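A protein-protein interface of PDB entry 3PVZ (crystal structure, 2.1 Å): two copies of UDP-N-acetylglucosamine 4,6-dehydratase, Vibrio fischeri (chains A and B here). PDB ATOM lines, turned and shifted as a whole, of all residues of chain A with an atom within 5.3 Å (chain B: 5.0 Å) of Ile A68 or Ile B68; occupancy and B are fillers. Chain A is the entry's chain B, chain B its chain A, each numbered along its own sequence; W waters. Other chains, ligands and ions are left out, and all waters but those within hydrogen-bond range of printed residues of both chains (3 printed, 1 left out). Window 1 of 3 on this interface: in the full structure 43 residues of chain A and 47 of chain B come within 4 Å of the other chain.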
ATOM      1  N   VAL A  66     -24.217  25.363  27.160  1.00  0.00           N
ATOM      2  CA  VAL A  66     -22.809  25.467  26.794  1.00  0.00           C
ATOM      3  C   VAL A  66     -22.139  24.090  26.825  1.00  0.00           C
ATOM      4  O   VAL A  66     -22.309  23.315  27.787  1.00  0.00           O
ATOM      5  CB  VAL A  66     -22.053  26.372  27.763  1.00  0.00           C
ATOM      6  CG1 VAL A  66     -20.593  26.450  27.349  1.00  0.00           C
ATOM      7  CG2 VAL A  66     -22.696  27.781  27.804  1.00  0.00           C
ATOM      8  N   ASP A  67     -21.436  23.769  25.741  1.00  0.00           N
ATOM      9  CA  ASP A  67     -20.745  22.528  25.617  1.00  0.00           C
ATOM     10  C   ASP A  67     -19.679  22.663  24.535  1.00  0.00           C
ATOM     11  O   ASP A  67     -19.890  23.311  23.491  1.00  0.00           O
ATOM     12  CB  ASP A  67     -21.714  21.410  25.277  1.00  0.00           C
ATOM     13  CG  ASP A  67     -21.105  20.033  25.477  1.00  0.00           C
ATOM     14  OD1 ASP A  67     -20.103  19.691  24.778  1.00  0.00           O
ATOM     15  OD2 ASP A  67     -21.621  19.276  26.336  1.00  0.00           O
ATOM     16  N   ILE A  68     -18.548  22.017  24.788  1.00  0.00           N
ATOM     17  CA  ILE A  68     -17.355  22.111  23.954  1.00  0.00           C
ATOM     18  C   ILE A  68     -17.552  21.332  22.630  1.00  0.00           C
ATOM     19  O   ILE A  68     -16.950  21.655  21.610  1.00  0.00           O
ATOM     20  CB  ILE A  68     -16.082  21.613  24.782  1.00  0.00           C
ATOM     21  CG1 ILE A  68     -14.823  22.316  24.302  1.00  0.00           C
ATOM     22  CG2 ILE A  68     -15.967  20.061  24.765  1.00  0.00           C
ATOM     23  CD1 ILE A  68     -13.551  21.790  24.910  1.00  0.00           C
ATOM     24  N   SER A  69     -18.465  20.363  22.634  1.00  0.00           N
ATOM     25  CA  SER A  69     -18.710  19.585  21.446  1.00  0.00           C
ATOM     26  C   SER A  69     -19.666  20.309  20.490  1.00  0.00           C
ATOM     27  O   SER A  69     -20.872  20.278  20.667  1.00  0.00           O
ATOM     28  CB  SER A  69     -19.269  18.213  21.780  1.00  0.00           C
ATOM     29  OG  SER A  69     -19.639  17.565  20.577  1.00  0.00           O
ATOM     30  N   GLU A  70     -19.106  20.926  19.457  1.00  0.00           N
ATOM     31  CA  GLU A  70     -19.901  21.574  18.428  1.00  0.00           C
ATOM     32  C   GLU A  70     -20.888  20.563  17.801  1.00  0.00           C
ATOM     33  O   GLU A  70     -22.091  20.830  17.724  1.00  0.00           O
ATOM     34  CB  GLU A  70     -18.928  22.147  17.383  1.00  0.00           C
ATOM     35  CG  GLU A  70     -19.572  22.923  16.277  1.00  0.00           C
ATOM     36  CD  GLU A  70     -18.653  23.157  15.088  1.00  0.00           C
ATOM     37  OE1 GLU A  70     -18.657  24.297  14.585  1.00  0.00           O
ATOM     38  OE2 GLU A  70     -17.962  22.215  14.630  1.00  0.00           O
ATOM     39  N   ALA A  95     -21.158  26.620  21.670  1.00  0.00           N
ATOM     40  CA  ALA A  95     -20.187  25.555  21.601  1.00  0.00           C
ATOM     41  C   ALA A  95     -18.831  26.089  22.148  1.00  0.00           C
ATOM     42  O   ALA A  95     -17.887  26.374  21.396  1.00  0.00           O
ATOM     43  CB  ALA A  95     -20.070  25.057  20.201  1.00  0.00           C
ATOM     44  N   LEU A  96     -18.773  26.234  23.463  1.00  0.00           N
ATOM     45  CA  LEU A  96     -17.635  26.842  24.122  1.00  0.00           C
ATOM     46  C   LEU A  96     -16.978  25.918  25.137  1.00  0.00           C
ATOM     47  O   LEU A  96     -17.628  25.051  25.738  1.00  0.00           O
ATOM     48  CB  LEU A  96     -18.057  28.123  24.837  1.00  0.00           C
ATOM     49  CG  LEU A  96     -18.663  29.235  23.975  1.00  0.00           C
ATOM     50  CD1 LEU A  96     -19.005  30.450  24.897  1.00  0.00           C
ATOM     51  CD2 LEU A  96     -17.708  29.646  22.800  1.00  0.00           C
ATOM     52  N   ASP A  97     -15.681  26.138  25.306  1.00  0.00           N
ATOM     53  CA  ASP A  97     -14.890  25.555  26.407  1.00  0.00           C
ATOM     54  C   ASP A  97     -15.028  26.467  27.620  1.00  0.00           C
ATOM     55  O   ASP A  97     -14.560  27.609  27.625  1.00  0.00           O
ATOM     56  CB  ASP A  97     -13.430  25.490  26.016  1.00  0.00           C
ATOM     57  CG  ASP A  97     -12.495  25.054  27.174  1.00  0.00           C
ATOM     58  OD1 ASP A  97     -12.914  24.539  28.257  1.00  0.00           O
ATOM     59  OD2 ASP A  97     -11.286  25.230  26.941  1.00  0.00           O
ATOM     60  N   ARG A 136      -5.735  17.790  32.356  1.00  0.00           N
ATOM     61  CA  ARG A 136      -7.009  18.288  31.796  1.00  0.00           C
ATOM     62  C   ARG A 136      -8.203  17.861  32.612  1.00  0.00           C
ATOM     63  O   ARG A 136      -9.110  18.624  32.852  1.00  0.00           O
ATOM     64  CB  ARG A 136      -7.203  17.871  30.329  1.00  0.00           C
ATOM     65  CG  ARG A 136      -8.373  18.670  29.649  1.00  0.00           C
ATOM     66  CD  ARG A 136      -8.764  18.148  28.313  1.00  0.00           C
ATOM     67  NE  ARG A 136     -10.120  18.564  27.940  1.00  0.00           N
ATOM     68  CZ  ARG A 136     -10.933  17.879  27.135  1.00  0.00           C
ATOM     69  NH1 ARG A 136     -12.172  18.317  26.934  1.00  0.00           N
ATOM     70  NH2 ARG A 136     -10.549  16.748  26.541  1.00  0.00           N
ATOM     71  N   VAL B  66      -4.776  12.949  18.922  1.00  0.00           N
ATOM     72  CA  VAL B  66      -5.183  13.978  19.897  1.00  0.00           C
ATOM     73  C   VAL B  66      -6.523  14.617  19.554  1.00  0.00           C
ATOM     74  O   VAL B  66      -6.734  15.053  18.449  1.00  0.00           O
ATOM     75  CB  VAL B  66      -4.143  15.061  19.931  1.00  0.00           C
ATOM     76  CG1 VAL B  66      -4.533  16.220  20.970  1.00  0.00           C
ATOM     77  CG2 VAL B  66      -2.776  14.464  20.319  1.00  0.00           C
ATOM     78  N   ASP B  67      -7.456  14.688  20.502  1.00  0.00           N
ATOM     79  CA  ASP B  67      -8.772  15.252  20.221  1.00  0.00           C
ATOM     80  C   ASP B  67      -9.433  15.538  21.538  1.00  0.00           C
ATOM     81  O   ASP B  67      -9.172  14.862  22.525  1.00  0.00           O
ATOM     82  CB  ASP B  67      -9.629  14.232  19.446  1.00  0.00           C
ATOM     83  CG  ASP B  67     -10.812  14.853  18.779  1.00  0.00           C
ATOM     84  OD1 ASP B  67     -11.793  15.264  19.478  1.00  0.00           O
ATOM     85  OD2 ASP B  67     -10.786  14.853  17.528  1.00  0.00           O
ATOM     86  N   ILE B  68     -10.298  16.530  21.564  1.00  0.00           N
ATOM     87  CA  ILE B  68     -10.926  16.882  22.815  1.00  0.00           C
ATOM     88  C   ILE B  68     -11.987  15.890  23.183  1.00  0.00           C
ATOM     89  O   ILE B  68     -12.274  15.769  24.352  1.00  0.00           O
ATOM     90  CB  ILE B  68     -11.535  18.305  22.853  1.00  0.00           C
ATOM     91  CG1 ILE B  68     -12.363  18.583  21.614  1.00  0.00           C
ATOM     92  CG2 ILE B  68     -10.475  19.338  22.959  1.00  0.00           C
ATOM     93  CD1 ILE B  68     -13.096  19.883  21.679  1.00  0.00           C
ATOM     94  N   SER B  69     -12.531  15.139  22.227  1.00  0.00           N
ATOM     95  CA  SER B  69     -13.595  14.200  22.553  1.00  0.00           C
ATOM     96  C   SER B  69     -13.032  12.874  23.092  1.00  0.00           C
ATOM     97  O   SER B  69     -12.563  12.061  22.324  1.00  0.00           O
ATOM     98  CB  SER B  69     -14.505  13.953  21.322  1.00  0.00           C
ATOM     99  OG  SER B  69     -15.392  12.876  21.581  1.00  0.00           O
ATOM    100  N   GLU B  70     -13.122  12.645  24.410  1.00  0.00           N
ATOM    101  CA  GLU B  70     -12.706  11.344  24.991  1.00  0.00           C
ATOM    102  C   GLU B  70     -13.651  10.264  24.580  1.00  0.00           C
ATOM    103  O   GLU B  70     -13.202   9.113  24.355  1.00  0.00           O
ATOM    104  CB  GLU B  70     -12.556  11.351  26.525  1.00  0.00           C
ATOM    105  CG  GLU B  70     -13.659  12.025  27.303  1.00  0.00           C
ATOM    106  CD  GLU B  70     -13.704  11.654  28.777  1.00  0.00           C
ATOM    107  OE1 GLU B  70     -12.727  11.104  29.345  1.00  0.00           O
ATOM    108  OE2 GLU B  70     -14.755  11.927  29.416  1.00  0.00           O
ATOM    109  N   ALA B  95      -6.643  12.862  25.036  1.00  0.00           N
ATOM    110  CA  ALA B  95      -7.864  13.664  24.914  1.00  0.00           C
ATOM    111  C   ALA B  95      -7.566  15.101  25.303  1.00  0.00           C
ATOM    112  O   ALA B  95      -8.027  15.574  26.336  1.00  0.00           O
ATOM    113  CB  ALA B  95      -8.994  13.080  25.819  1.00  0.00           C
ATOM    114  N   LEU B  96      -6.800  15.786  24.471  1.00  0.00           N
ATOM    115  CA  LEU B  96      -6.301  17.110  24.778  1.00  0.00           C
ATOM    116  C   LEU B  96      -6.889  18.136  23.781  1.00  0.00           C
ATOM    117  O   LEU B  96      -7.250  17.801  22.644  1.00  0.00           O
ATOM    118  CB  LEU B  96      -4.791  17.098  24.669  1.00  0.00           C
ATOM    119  CG  LEU B  96      -3.913  16.221  25.569  1.00  0.00           C
ATOM    120  CD1 LEU B  96      -2.384  16.396  25.181  1.00  0.00           C
ATOM    121  CD2 LEU B  96      -4.172  16.561  26.978  1.00  0.00           C
ATOM    122  N   ASP B  97      -7.071  19.346  24.269  1.00  0.00           N
ATOM    123  CA  ASP B  97      -7.420  20.474  23.495  1.00  0.00           C
ATOM    124  C   ASP B  97      -6.104  21.114  23.024  1.00  0.00           C
ATOM    125  O   ASP B  97      -5.236  21.456  23.834  1.00  0.00           O
ATOM    126  CB  ASP B  97      -8.154  21.450  24.391  1.00  0.00           C
ATOM    127  CG  ASP B  97      -8.666  22.679  23.639  1.00  0.00           C
ATOM    128  OD1 ASP B  97      -7.908  23.279  22.810  1.00  0.00           O
ATOM    129  OD2 ASP B  97      -9.841  23.054  23.892  1.00  0.00           O
ATOM    130  N   ARG B 136     -13.926  31.466  19.111  1.00  0.00           N
ATOM    131  CA  ARG B 136     -13.385  30.135  19.282  1.00  0.00           C
ATOM    132  C   ARG B 136     -13.008  29.499  17.935  1.00  0.00           C
ATOM    133  O   ARG B 136     -12.049  28.782  17.838  1.00  0.00           O
ATOM    134  CB  ARG B 136     -14.347  29.221  20.066  1.00  0.00           C
ATOM    135  CG  ARG B 136     -13.774  27.837  20.205  1.00  0.00           C
ATOM    136  CD  ARG B 136     -14.609  26.884  21.018  1.00  0.00           C
ATOM    137  NE  ARG B 136     -13.991  25.566  20.948  1.00  0.00           N
ATOM    138  CZ  ARG B 136     -14.642  24.412  20.807  1.00  0.00           C
ATOM    139  NH1 ARG B 136     -15.955  24.361  20.703  1.00  0.00           N
ATOM    140  NH2 ARG B 136     -13.973  23.295  20.696  1.00  0.00           N
HETATM  141  O   HOH W   1     -14.236  16.473  26.205  1.00  0.00           O
HETATM  142  O   HOH W   2     -10.415  22.648  26.561  1.00  0.00           O
HETATM  143  O   HOH W   3     -17.849  14.919  20.783  1.00  0.00           O
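The backbone carbonyl oxygen (O) of Ile B68 sits at hydrogen-bond distance from the guanidinium group (NH2) of Arg A136, 3.0 Å away.
The backbone carbonyl oxygen of Ala B95 sits at hydrogen-bond distance from the guanidinium group of Arg A136.
NH1 of Arg B136 sits at hydrogen-bond distance from O of Ile A68, 3.0 Å away.
The guanidinium group of Arg B136 sits at hydrogen-bond distance from the backbone carbonyl oxygen of Ala A95, at 2.9 Å.
The backbone NH (N) of Ile B68 is in hydrogen-bond range of the backbone carbonyl oxygen (O) of Leu B96 (3.5 Å).
The backbone NH (N) of Ile A68 sits at hydrogen-bond distance from the backbone carbonyl oxygen (O) of Leu A96, at 3.3 Å.
Among the printed residues, merely in contact across the chains: Ile A68 with Ile B68.
Of chain B, only Ile B68 and Arg B136 come within 4 Å of Ile A68.
Of chain A, only Ile A68 (3.8 Å) and Arg A136 (3.0 Å) come within 4 Å of Ile B68.
Of the printed residues of chain B, Ala A95 touches Arg B136.
Of the printed residues of chain A, Ala B95 touches Arg A136.
Asp A67 touches none of the printed residues of chain B.
Asp B97 touches none of the printed residues of chain A.
The nearest residue of chain B that does not touch Ile A68 is Asp B97 (4.05 Å).
Hydrophobic or aromatic side chains of chain B that line the printed part of chain A: Ile B68.
Hydrophobic or aromatic side chains of chain A within 4 Å of the printed part of chain B: Ile A68.
Among the printed residues, no Asp or Glu carboxylate lies within 4 Å of a Lys or Arg side-chain nitrogen of the other chain.
Ile B68 touches its own counterpart, Ile A68.
Ile A68 touches Arg B136, and with the chains exchanged Arg A136 touches Ile B68.
Ala A95 touches Arg B136, and with the chains exchanged Arg A136 touches Ala B95.
Positions printed for both chains: 66, 67, 68, 69, 70, 95, 96, 97 and 136.
Of the 5 pairs that touch across the chains among the printed residues, 5 have their exchanged pair printed and touching as well.
Water W2 lies within hydrogen-bond range of the side-chain carboxylate of Asp A97 (2.8 Å) and the side-chain carboxylate of Asp B97 (2.8 Å).
Water W1 bridges the backbone carbonyl oxygen of Ile B68 and the guanidinium group of Arg A136.
Water W3 lies within hydrogen-bond range of OG of Ser A69 (3.2 Å) and OG of Ser B69 (3.3 Å).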
